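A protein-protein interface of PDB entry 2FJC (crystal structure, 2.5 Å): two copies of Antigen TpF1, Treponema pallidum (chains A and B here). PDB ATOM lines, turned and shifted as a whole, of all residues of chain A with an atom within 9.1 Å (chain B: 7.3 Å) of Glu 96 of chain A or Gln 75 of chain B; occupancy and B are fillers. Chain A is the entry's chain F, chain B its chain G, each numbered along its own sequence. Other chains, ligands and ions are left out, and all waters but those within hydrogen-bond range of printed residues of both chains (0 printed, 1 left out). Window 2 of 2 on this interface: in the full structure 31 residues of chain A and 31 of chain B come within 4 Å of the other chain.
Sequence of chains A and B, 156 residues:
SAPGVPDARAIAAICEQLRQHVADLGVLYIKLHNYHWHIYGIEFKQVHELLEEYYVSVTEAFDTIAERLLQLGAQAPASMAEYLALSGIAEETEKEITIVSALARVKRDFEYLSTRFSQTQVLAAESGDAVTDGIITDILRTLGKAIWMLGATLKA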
ATOM      1  N   ASN A  34      -2.799 -11.790 -16.983  1.00  0.00           N
ATOM      2  CA  ASN A  34      -2.307 -11.169 -15.771  1.00  0.00           C
ATOM      3  C   ASN A  34      -3.392 -10.247 -15.217  1.00  0.00           C
ATOM      4  O   ASN A  34      -3.772 -10.358 -14.044  1.00  0.00           O
ATOM      5  CB  ASN A  34      -1.032 -10.380 -16.069  1.00  0.00           C
ATOM      6  CG  ASN A  34      -0.316  -9.937 -14.817  1.00  0.00           C
ATOM      7  OD1 ASN A  34      -0.934  -9.463 -13.869  1.00  0.00           O
ATOM      8  ND2 ASN A  34       0.995 -10.075 -14.813  1.00  0.00           N
ATOM      9  N   TYR A  35      -3.901  -9.340 -16.054  1.00  0.00           N
ATOM     10  CA  TYR A  35      -4.955  -8.423 -15.612  1.00  0.00           C
ATOM     11  C   TYR A  35      -6.212  -9.202 -15.258  1.00  0.00           C
ATOM     12  O   TYR A  35      -6.872  -8.931 -14.254  1.00  0.00           O
ATOM     13  CB  TYR A  35      -5.269  -7.401 -16.705  1.00  0.00           C
ATOM     14  CG  TYR A  35      -4.071  -6.559 -17.067  1.00  0.00           C
ATOM     15  CD1 TYR A  35      -3.197  -6.092 -16.074  1.00  0.00           C
ATOM     16  CD2 TYR A  35      -3.792  -6.247 -18.390  1.00  0.00           C
ATOM     17  CE1 TYR A  35      -2.075  -5.346 -16.397  1.00  0.00           C
ATOM     18  CE2 TYR A  35      -2.680  -5.500 -18.722  1.00  0.00           C
ATOM     19  CZ  TYR A  35      -1.821  -5.054 -17.721  1.00  0.00           C
ATOM     20  OH  TYR A  35      -0.699  -4.334 -18.054  1.00  0.00           O
ATOM     21  N   HIS A  36      -6.524 -10.181 -16.097  1.00  0.00           N
ATOM     22  CA  HIS A  36      -7.685 -11.041 -15.911  1.00  0.00           C
ATOM     23  C   HIS A  36      -7.698 -11.623 -14.505  1.00  0.00           C
ATOM     24  O   HIS A  36      -8.742 -11.669 -13.857  1.00  0.00           O
ATOM     25  CB  HIS A  36      -7.634 -12.172 -16.937  1.00  0.00           C
ATOM     26  CG  HIS A  36      -8.769 -13.146 -16.849  1.00  0.00           C
ATOM     27  ND1 HIS A  36     -10.063 -12.821 -17.202  1.00  0.00           N
ATOM     28  CD2 HIS A  36      -8.789 -14.458 -16.518  1.00  0.00           C
ATOM     29  CE1 HIS A  36     -10.829 -13.894 -17.097  1.00  0.00           C
ATOM     30  NE2 HIS A  36     -10.079 -14.901 -16.683  1.00  0.00           N
ATOM     31  N   TRP A  37      -6.530 -12.056 -14.037  1.00  0.00           N
ATOM     32  CA  TRP A  37      -6.409 -12.670 -12.722  1.00  0.00           C
ATOM     33  C   TRP A  37      -6.203 -11.725 -11.551  1.00  0.00           C
ATOM     34  O   TRP A  37      -6.718 -11.970 -10.465  1.00  0.00           O
ATOM     35  CB  TRP A  37      -5.236 -13.654 -12.689  1.00  0.00           C
ATOM     36  CG  TRP A  37      -5.292 -14.775 -13.665  1.00  0.00           C
ATOM     37  CD1 TRP A  37      -6.382 -15.527 -13.991  1.00  0.00           C
ATOM     38  CD2 TRP A  37      -4.182 -15.336 -14.381  1.00  0.00           C
ATOM     39  NE1 TRP A  37      -6.022 -16.527 -14.865  1.00  0.00           N
ATOM     40  CE2 TRP A  37      -4.677 -16.432 -15.122  1.00  0.00           C
ATOM     41  CE3 TRP A  37      -2.818 -15.021 -14.467  1.00  0.00           C
ATOM     42  CZ2 TRP A  37      -3.852 -17.219 -15.941  1.00  0.00           C
ATOM     43  CZ3 TRP A  37      -2.001 -15.803 -15.279  1.00  0.00           C
ATOM     44  CH2 TRP A  37      -2.526 -16.890 -16.006  1.00  0.00           C
ATOM     45  N   HIS A  38      -5.455 -10.650 -11.765  1.00  0.00           N
ATOM     46  CA  HIS A  38      -5.123  -9.760 -10.661  1.00  0.00           C
ATOM     47  C   HIS A  38      -5.850  -8.436 -10.463  1.00  0.00           C
ATOM     48  O   HIS A  38      -5.532  -7.699  -9.522  1.00  0.00           O
ATOM     49  CB  HIS A  38      -3.605  -9.523 -10.675  1.00  0.00           C
ATOM     50  CG  HIS A  38      -2.809 -10.792 -10.690  1.00  0.00           C
ATOM     51  ND1 HIS A  38      -1.867 -11.071 -11.657  1.00  0.00           N
ATOM     52  CD2 HIS A  38      -2.863 -11.885  -9.890  1.00  0.00           C
ATOM     53  CE1 HIS A  38      -1.377 -12.284 -11.455  1.00  0.00           C
ATOM     54  NE2 HIS A  38      -1.965 -12.797 -10.388  1.00  0.00           N
ATOM     55  N   ILE A  39      -6.809  -8.116 -11.325  1.00  0.00           N
ATOM     56  CA  ILE A  39      -7.543  -6.875 -11.137  1.00  0.00           C
ATOM     57  C   ILE A  39      -8.426  -7.077  -9.916  1.00  0.00           C
ATOM     58  O   ILE A  39      -8.678  -8.201  -9.499  1.00  0.00           O
ATOM     59  CB  ILE A  39      -8.465  -6.547 -12.329  1.00  0.00           C
ATOM     60  CG1 ILE A  39      -9.401  -7.729 -12.601  1.00  0.00           C
ATOM     61  CG2 ILE A  39      -7.636  -6.169 -13.545  1.00  0.00           C
ATOM     62  CD1 ILE A  39     -10.503  -7.427 -13.584  1.00  0.00           C
ATOM     63  N   TYR A  40      -8.878  -5.981  -9.335  1.00  0.00           N
ATOM     64  CA  TYR A  40      -9.765  -6.042  -8.190  1.00  0.00           C
ATOM     65  C   TYR A  40     -10.576  -4.755  -8.227  1.00  0.00           C
ATOM     66  O   TYR A  40     -10.141  -3.749  -8.798  1.00  0.00           O
ATOM     67  CB  TYR A  40      -8.984  -6.164  -6.871  1.00  0.00           C
ATOM     68  CG  TYR A  40      -8.164  -4.949  -6.510  1.00  0.00           C
ATOM     69  CD1 TYR A  40      -6.848  -4.822  -6.940  1.00  0.00           C
ATOM     70  CD2 TYR A  40      -8.713  -3.916  -5.750  1.00  0.00           C
ATOM     71  CE1 TYR A  40      -6.095  -3.699  -6.623  1.00  0.00           C
ATOM     72  CE2 TYR A  40      -7.965  -2.784  -5.428  1.00  0.00           C
ATOM     73  CZ  TYR A  40      -6.659  -2.687  -5.870  1.00  0.00           C
ATOM     74  OH  TYR A  40      -5.914  -1.578  -5.555  1.00  0.00           O
ATOM     75  N   GLY A  41     -11.760  -4.792  -7.632  1.00  0.00           N
ATOM     76  CA  GLY A  41     -12.613  -3.622  -7.634  1.00  0.00           C
ATOM     77  C   GLY A  41     -14.043  -4.057  -7.857  1.00  0.00           C
ATOM     78  O   GLY A  41     -14.307  -5.190  -8.267  1.00  0.00           O
ATOM     79  N   GLU A  92       3.744  -7.464 -17.956  1.00  0.00           N
ATOM     80  CA  GLU A  92       3.268  -6.896 -16.708  1.00  0.00           C
ATOM     81  C   GLU A  92       3.959  -7.656 -15.583  1.00  0.00           C
ATOM     82  O   GLU A  92       3.770  -8.867 -15.423  1.00  0.00           O
ATOM     83  CB  GLU A  92       1.754  -7.051 -16.580  1.00  0.00           C
ATOM     84  CG  GLU A  92       1.203  -6.409 -15.330  1.00  0.00           C
ATOM     85  CD  GLU A  92       1.568  -4.942 -15.242  1.00  0.00           C
ATOM     86  OE1 GLU A  92       0.967  -4.128 -15.973  1.00  0.00           O
ATOM     87  OE2 GLU A  92       2.472  -4.598 -14.453  1.00  0.00           O
ATOM     88  N   THR A  93       4.762  -6.942 -14.804  1.00  0.00           N
ATOM     89  CA  THR A  93       5.499  -7.563 -13.711  1.00  0.00           C
ATOM     90  C   THR A  93       4.758  -7.513 -12.399  1.00  0.00           C
ATOM     91  O   THR A  93       5.024  -8.313 -11.505  1.00  0.00           O
ATOM     92  CB  THR A  93       6.861  -6.894 -13.500  1.00  0.00           C
ATOM     93  OG1 THR A  93       6.667  -5.500 -13.216  1.00  0.00           O
ATOM     94  CG2 THR A  93       7.730  -7.055 -14.745  1.00  0.00           C
ATOM     95  N   GLU A  94       3.831  -6.579 -12.267  1.00  0.00           N
ATOM     96  CA  GLU A  94       3.104  -6.498 -11.021  1.00  0.00           C
ATOM     97  C   GLU A  94       1.818  -7.291 -11.071  1.00  0.00           C
ATOM     98  O   GLU A  94       1.278  -7.574 -12.138  1.00  0.00           O
ATOM     99  CB  GLU A  94       2.826  -5.038 -10.639  1.00  0.00           C
ATOM    100  CG  GLU A  94       1.919  -4.275 -11.571  1.00  0.00           C
ATOM    101  CD  GLU A  94       1.852  -2.791 -11.226  1.00  0.00           C
ATOM    102  OE1 GLU A  94       2.890  -2.103 -11.349  1.00  0.00           O
ATOM    103  OE2 GLU A  94       0.763  -2.317 -10.832  1.00  0.00           O
ATOM    104  N   LYS A  95       1.366  -7.692  -9.894  1.00  0.00           N
ATOM    105  CA  LYS A  95       0.134  -8.438  -9.735  1.00  0.00           C
ATOM    106  C   LYS A  95      -0.669  -7.543  -8.804  1.00  0.00           C
ATOM    107  O   LYS A  95      -0.117  -6.595  -8.236  1.00  0.00           O
ATOM    108  CB  LYS A  95       0.436  -9.804  -9.125  1.00  0.00           C
ATOM    109  CG  LYS A  95       1.341 -10.622 -10.032  1.00  0.00           C
ATOM    110  CD  LYS A  95       1.822 -11.914  -9.403  1.00  0.00           C
ATOM    111  CE  LYS A  95       2.755 -12.665 -10.357  1.00  0.00           C
ATOM    112  NZ  LYS A  95       3.959 -11.869 -10.746  1.00  0.00           N
ATOM    113  N   GLU A  96      -1.956  -7.819  -8.641  1.00  0.00           N
ATOM    114  CA  GLU A  96      -2.792  -6.959  -7.814  1.00  0.00           C
ATOM    115  C   GLU A  96      -2.748  -5.579  -8.465  1.00  0.00           C
ATOM    116  O   GLU A  96      -1.833  -4.790  -8.220  1.00  0.00           O
ATOM    117  CB  GLU A  96      -2.265  -6.857  -6.380  1.00  0.00           C
ATOM    118  CG  GLU A  96      -3.072  -5.895  -5.536  1.00  0.00           C
ATOM    119  CD  GLU A  96      -2.693  -5.915  -4.073  1.00  0.00           C
ATOM    120  OE1 GLU A  96      -2.799  -6.991  -3.443  1.00  0.00           O
ATOM    121  OE2 GLU A  96      -2.295  -4.849  -3.552  1.00  0.00           O
ATOM    122  N   ILE A  97      -3.741  -5.298  -9.300  1.00  0.00           N
ATOM    123  CA  ILE A  97      -3.801  -4.028 -10.001  1.00  0.00           C
ATOM    124  C   ILE A  97      -5.218  -3.473 -10.073  1.00  0.00           C
ATOM    125  O   ILE A  97      -6.194  -4.217 -10.124  1.00  0.00           O
ATOM    126  CB  ILE A  97      -3.230  -4.183 -11.440  1.00  0.00           C
ATOM    127  CG1 ILE A  97      -3.274  -2.844 -12.177  1.00  0.00           C
ATOM    128  CG2 ILE A  97      -4.011  -5.242 -12.196  1.00  0.00           C
ATOM    129  CD1 ILE A  97      -2.599  -2.886 -13.534  1.00  0.00           C
ATOM    130  N   THR A  98      -5.316  -2.152 -10.059  1.00  0.00           N
ATOM    131  CA  THR A  98      -6.592  -1.459 -10.150  1.00  0.00           C
ATOM    132  C   THR A  98      -7.237  -1.723 -11.513  1.00  0.00           C
ATOM    133  O   THR A  98      -6.548  -1.950 -12.511  1.00  0.00           O
ATOM    134  CB  THR A  98      -6.385   0.072  -9.989  1.00  0.00           C
ATOM    135  OG1 THR A  98      -6.092   0.374  -8.619  1.00  0.00           O
ATOM    136  CG2 THR A  98      -7.612   0.834 -10.401  1.00  0.00           C
ATOM    137  N   ILE A  99      -8.560  -1.682 -11.558  1.00  0.00           N
ATOM    138  CA  ILE A  99      -9.261  -1.898 -12.811  1.00  0.00           C
ATOM    139  C   ILE A  99      -8.954  -0.798 -13.831  1.00  0.00           C
ATOM    140  O   ILE A  99      -8.624  -1.098 -14.983  1.00  0.00           O
ATOM    141  CB  ILE A  99     -10.777  -2.014 -12.570  1.00  0.00           C
ATOM    142  CG1 ILE A  99     -11.078  -3.395 -11.971  1.00  0.00           C
ATOM    143  CG2 ILE A  99     -11.543  -1.791 -13.871  1.00  0.00           C
ATOM    144  CD1 ILE A  99     -12.530  -3.614 -11.567  1.00  0.00           C
ATOM    145  N   SER A 101      -6.418   1.088 -13.925  1.00  0.00           N
ATOM    146  CA  SER A 101      -4.996   0.983 -14.239  1.00  0.00           C
ATOM    147  C   SER A 101      -4.769  -0.113 -15.300  1.00  0.00           C
ATOM    148  O   SER A 101      -4.015   0.069 -16.264  1.00  0.00           O
ATOM    149  CB  SER A 101      -4.227   0.651 -12.954  1.00  0.00           C
ATOM    150  OG  SER A 101      -2.839   0.850 -13.116  1.00  0.00           O
ATOM    151  N   ALA A 102      -5.435  -1.249 -15.124  1.00  0.00           N
ATOM    152  CA  ALA A 102      -5.292  -2.349 -16.064  1.00  0.00           C
ATOM    153  C   ALA A 102      -5.863  -1.990 -17.438  1.00  0.00           C
ATOM    154  O   ALA A 102      -5.218  -2.213 -18.471  1.00  0.00           O
ATOM    155  CB  ALA A 102      -5.975  -3.586 -15.524  1.00  0.00           C
ATOM    156  N   ARG A 105      -3.777   0.344 -19.412  1.00  0.00           N
ATOM    157  CA  ARG A 105      -2.621  -0.326 -19.982  1.00  0.00           C
ATOM    158  C   ARG A 105      -2.976  -1.155 -21.210  1.00  0.00           C
ATOM    159  O   ARG A 105      -2.222  -1.150 -22.178  1.00  0.00           O
ATOM    160  CB  ARG A 105      -1.930  -1.188 -18.928  1.00  0.00           C
ATOM    161  CG  ARG A 105      -1.321  -0.366 -17.810  1.00  0.00           C
ATOM    162  CD  ARG A 105      -0.680  -1.212 -16.728  1.00  0.00           C
ATOM    163  NE  ARG A 105      -0.422  -0.402 -15.536  1.00  0.00           N
ATOM    164  CZ  ARG A 105       0.126  -0.857 -14.407  1.00  0.00           C
ATOM    165  NH1 ARG A 105       0.494  -2.130 -14.293  1.00  0.00           N
ATOM    166  NH2 ARG A 105       0.295  -0.038 -13.377  1.00  0.00           N
ATOM    167  N   CYS B  15       0.727 -24.573  -3.613  1.00  0.00           N
ATOM    168  CA  CYS B  15       0.812 -23.362  -4.428  1.00  0.00           C
ATOM    169  C   CYS B  15       2.076 -23.357  -5.265  1.00  0.00           C
ATOM    170  O   CYS B  15       2.070 -22.917  -6.415  1.00  0.00           O
ATOM    171  CB  CYS B  15       0.772 -22.101  -3.556  1.00  0.00           C
ATOM    172  SG  CYS B  15      -0.870 -21.710  -2.914  1.00  0.00           S
ATOM    173  N   ARG B  19       2.018 -23.086  -9.258  1.00  0.00           N
ATOM    174  CA  ARG B  19       2.766 -22.051  -9.962  1.00  0.00           C
ATOM    175  C   ARG B  19       3.565 -22.685 -11.092  1.00  0.00           C
ATOM    176  O   ARG B  19       3.673 -22.121 -12.186  1.00  0.00           O
ATOM    177  CB  ARG B  19       3.740 -21.339  -9.024  1.00  0.00           C
ATOM    178  CG  ARG B  19       3.104 -20.509  -7.925  1.00  0.00           C
ATOM    179  CD  ARG B  19       4.199 -19.836  -7.105  1.00  0.00           C
ATOM    180  NE  ARG B  19       5.182 -19.178  -7.970  1.00  0.00           N
ATOM    181  CZ  ARG B  19       4.942 -18.082  -8.690  1.00  0.00           C
ATOM    182  NH1 ARG B  19       3.746 -17.500  -8.650  1.00  0.00           N
ATOM    183  NH2 ARG B  19       5.895 -17.573  -9.467  1.00  0.00           N
ATOM    184  N   ALA B  66      -4.508 -21.600 -12.600  1.00  0.00           N
ATOM    185  CA  ALA B  66      -4.083 -20.269 -12.193  1.00  0.00           C
ATOM    186  C   ALA B  66      -5.117 -19.686 -11.242  1.00  0.00           C
ATOM    187  O   ALA B  66      -4.773 -19.055 -10.242  1.00  0.00           O
ATOM    188  CB  ALA B  66      -3.938 -19.369 -13.413  1.00  0.00           C
ATOM    189  N   LEU B  69      -4.990 -21.145  -7.842  1.00  0.00           N
ATOM    190  CA  LEU B  69      -3.870 -20.549  -7.154  1.00  0.00           C
ATOM    191  C   LEU B  69      -4.351 -19.253  -6.512  1.00  0.00           C
ATOM    192  O   LEU B  69      -4.052 -18.979  -5.345  1.00  0.00           O
ATOM    193  CB  LEU B  69      -2.763 -20.278  -8.165  1.00  0.00           C
ATOM    194  CG  LEU B  69      -1.357 -19.940  -7.693  1.00  0.00           C
ATOM    195  CD1 LEU B  69      -0.913 -20.941  -6.640  1.00  0.00           C
ATOM    196  CD2 LEU B  69      -0.423 -19.980  -8.894  1.00  0.00           C
ATOM    197  N   LEU B  70      -5.114 -18.468  -7.273  1.00  0.00           N
ATOM    198  CA  LEU B  70      -5.650 -17.196  -6.781  1.00  0.00           C
ATOM    199  C   LEU B  70      -6.555 -17.422  -5.586  1.00  0.00           C
ATOM    200  O   LEU B  70      -6.500 -16.677  -4.605  1.00  0.00           O
ATOM    201  CB  LEU B  70      -6.439 -16.477  -7.878  1.00  0.00           C
ATOM    202  CG  LEU B  70      -5.627 -16.030  -9.096  1.00  0.00           C
ATOM    203  CD1 LEU B  70      -6.563 -15.476 -10.161  1.00  0.00           C
ATOM    204  CD2 LEU B  70      -4.599 -14.982  -8.677  1.00  0.00           C
ATOM    205  N   LEU B  72      -6.396 -19.810  -3.489  1.00  0.00           N
ATOM    206  CA  LEU B  72      -5.592 -20.231  -2.356  1.00  0.00           C
ATOM    207  C   LEU B  72      -4.830 -19.068  -1.722  1.00  0.00           C
ATOM    208  O   LEU B  72      -4.020 -19.263  -0.817  1.00  0.00           O
ATOM    209  CB  LEU B  72      -4.626 -21.334  -2.792  1.00  0.00           C
ATOM    210  CG  LEU B  72      -5.307 -22.677  -3.070  1.00  0.00           C
ATOM    211  CD1 LEU B  72      -4.283 -23.704  -3.521  1.00  0.00           C
ATOM    212  CD2 LEU B  72      -6.017 -23.148  -1.804  1.00  0.00           C
ATOM    213  N   GLY B  73      -5.088 -17.858  -2.207  1.00  0.00           N
ATOM    214  CA  GLY B  73      -4.440 -16.686  -1.646  1.00  0.00           C
ATOM    215  C   GLY B  73      -3.131 -16.280  -2.287  1.00  0.00           C
ATOM    216  O   GLY B  73      -2.507 -15.311  -1.858  1.00  0.00           O
ATOM    217  N   ALA B  74      -2.699 -17.010  -3.307  1.00  0.00           N
ATOM    218  CA  ALA B  74      -1.448 -16.673  -3.974  1.00  0.00           C
ATOM    219  C   ALA B  74      -1.720 -15.887  -5.258  1.00  0.00           C
ATOM    220  O   ALA B  74      -2.870 -15.713  -5.664  1.00  0.00           O
ATOM    221  CB  ALA B  74      -0.673 -17.940  -4.289  1.00  0.00           C
ATOM    222  N   GLN B  75      -0.662 -15.386  -5.882  1.00  0.00           N
ATOM    223  CA  GLN B  75      -0.821 -14.661  -7.132  1.00  0.00           C
ATOM    224  C   GLN B  75      -0.215 -15.580  -8.166  1.00  0.00           C
ATOM    225  O   GLN B  75       0.747 -16.296  -7.880  1.00  0.00           O
ATOM    226  CB  GLN B  75      -0.103 -13.312  -7.097  1.00  0.00           C
ATOM    227  CG  GLN B  75      -0.484 -12.461  -5.891  1.00  0.00           C
ATOM    228  CD  GLN B  75      -0.379 -10.968  -6.162  1.00  0.00           C
ATOM    229  OE1 GLN B  75      -1.273 -10.373  -6.775  1.00  0.00           O
ATOM    230  NE2 GLN B  75       0.716 -10.353  -5.712  1.00  0.00           N
ATOM    231  N   ALA B  76      -0.792 -15.587  -9.359  1.00  0.00           N
ATOM    232  CA  ALA B  76      -0.316 -16.471 -10.409  1.00  0.00           C
ATOM    233  C   ALA B  76       0.796 -15.877 -11.249  1.00  0.00           C
ATOM    234  O   ALA B  76       0.817 -14.673 -11.519  1.00  0.00           O
ATOM    235  CB  ALA B  76      -1.475 -16.870 -11.305  1.00  0.00           C
ATOM    236  N   PRO B  77       1.759 -16.713 -11.655  1.00  0.00           N
ATOM    237  CA  PRO B  77       2.845 -16.192 -12.481  1.00  0.00           C
ATOM    238  C   PRO B  77       2.157 -15.744 -13.766  1.00  0.00           C
ATOM    239  O   PRO B  77       1.371 -16.494 -14.348  1.00  0.00           O
ATOM    240  CB  PRO B  77       3.748 -17.409 -12.660  1.00  0.00           C
ATOM    241  CG  PRO B  77       2.783 -18.574 -12.566  1.00  0.00           C
ATOM    242  CD  PRO B  77       1.911 -18.158 -11.418  1.00  0.00           C
ATOM    243  N   ALA B  78       2.431 -14.521 -14.202  1.00  0.00           N
ATOM    244  CA  ALA B  78       1.765 -14.008 -15.386  1.00  0.00           C
ATOM    245  C   ALA B  78       2.651 -13.250 -16.359  1.00  0.00           C
ATOM    246  O   ALA B  78       2.394 -12.095 -16.675  1.00  0.00           O
ATOM    247  CB  ALA B  78       0.596 -13.133 -14.953  1.00  0.00           C
ATOM    248  N   GLU B  82       8.632 -15.102 -16.261  1.00  0.00           N
ATOM    249  CA  GLU B  82       8.450 -15.989 -15.119  1.00  0.00           C
ATOM    250  C   GLU B  82       8.257 -17.430 -15.572  1.00  0.00           C
ATOM    251  O   GLU B  82       8.803 -18.349 -14.967  1.00  0.00           O
ATOM    252  CB  GLU B  82       7.235 -15.583 -14.280  1.00  0.00           C
ATOM    253  CG  GLU B  82       7.231 -14.154 -13.797  1.00  0.00           C
ATOM    254  CD  GLU B  82       5.926 -13.799 -13.099  1.00  0.00           C
ATOM    255  OE1 GLU B  82       5.765 -14.165 -11.913  1.00  0.00           O
ATOM    256  OE2 GLU B  82       5.054 -13.168 -13.745  1.00  0.00           O
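A ring nitrogen (NE2) of His 38 of chain A lies within hydrogen-bond range of the backbone NH (N) of Ala 76 of chain B. The backbone NH of Glu 96 of chain A lies within hydrogen-bond range of the side-chain amide oxygen of Gln 75 of chain B, at 3.2 Å. O of Ala 78 of chain B sits at hydrogen-bond distance from ND2 of Asn 34 of chain A (3.1 Å). OE1 of Glu 82 of chain B is in salt-bridge range of NZ of Lys 95 of chain A (3.1 Å).
OE1 of Glu 92 of chain A lies within salt-bridge range of NH1 of Arg 105 of chain A (2.7 Å). O of His 38 of chain A lies within hydrogen-bond range of N of Ile 97 of chain A. N of Ala 78 of chain B lies within hydrogen-bond range of OE2 of Glu 82 of chain B (3.0 Å). The guanidinium group of Arg 19 of chain B sits at hydrogen-bond distance from the backbone carbonyl oxygen of Gln 75 of chain B (3.3 Å). O of Glu 92 of chain A sits at hydrogen-bond distance from ND2 of Asn 34 of chain A, at 3.1 Å. The side-chain carboxylate (OE2) of Glu 92 of chain A lies close to the backbone NH (N) of Glu 94 of chain A (3.2 Å).
Trp 37 of chain A touches Ala 66 of chain B. Leu 70 of chain B touches Trp 37 of chain A (CD1 to CB, 3.4 Å). CE3 of Trp 37 of chain A touches CB of Ala 76 of chain B, 3.9 Å away. Pro 77 of chain B touches Trp 37 of chain A. Ala 78 of chain B touches Trp 37 of chain A. His 38 of chain A touches Leu 70 of chain B. Gln 75 of chain B touches His 38 of chain A. O of Ala 78 of chain B touches O of Glu 92 of chain A, at 3.7 Å. Lys 95 of chain A touches Gln 75 of chain B (CB to OE1, 3.0 Å). Lys 95 of chain A touches Ala 76 of chain B (CE to O, 3.0 Å).
Glu 96 of chain A touches just one residue of chain B: Gln 75. Of chain A, only His 38, Lys 95 and Glu 96 come within 4 Å of Gln 75 of chain B. No residue of chain A comes within 4 Å of Ala 74 of chain B. Of the printed residues of chain B, His 38 of chain A touches Leu 70, Gln 75 and Ala 76. Of the printed residues of chain A, Leu 70 of chain B touches Trp 37 (3.4 Å) and His 38 (3.8 Å). Of the printed residues of chain A, Pro 77 of chain B touches Trp 37 (3.6 Å). Of the printed residues of chain A, Glu 82 of chain B touches Lys 95 (3.1 Å). Of the printed residues of chain B, Lys 95 of chain A touches Gln 75, Ala 76 and Glu 82.
Hydrophobic or aromatic side chains of chain B that line the printed part of chain A: Ala 66, Leu 70, Ala 76 and Ala 78. Hydrophobic or aromatic side chains of chain A within 4 Å of the printed part of chain B: Trp 37 and His 38. Among the printed residues, Asp or Glu carboxylates within 4 Å of a Lys or Arg side-chain nitrogen of the other chain: Lys 95 of chain A with Glu 82 of chain B (3.1 Å).
No position is printed for both chains. Of the 14 pairs that touch across the chains among the printed residues, none has its exchanged pair printed and touching as well.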
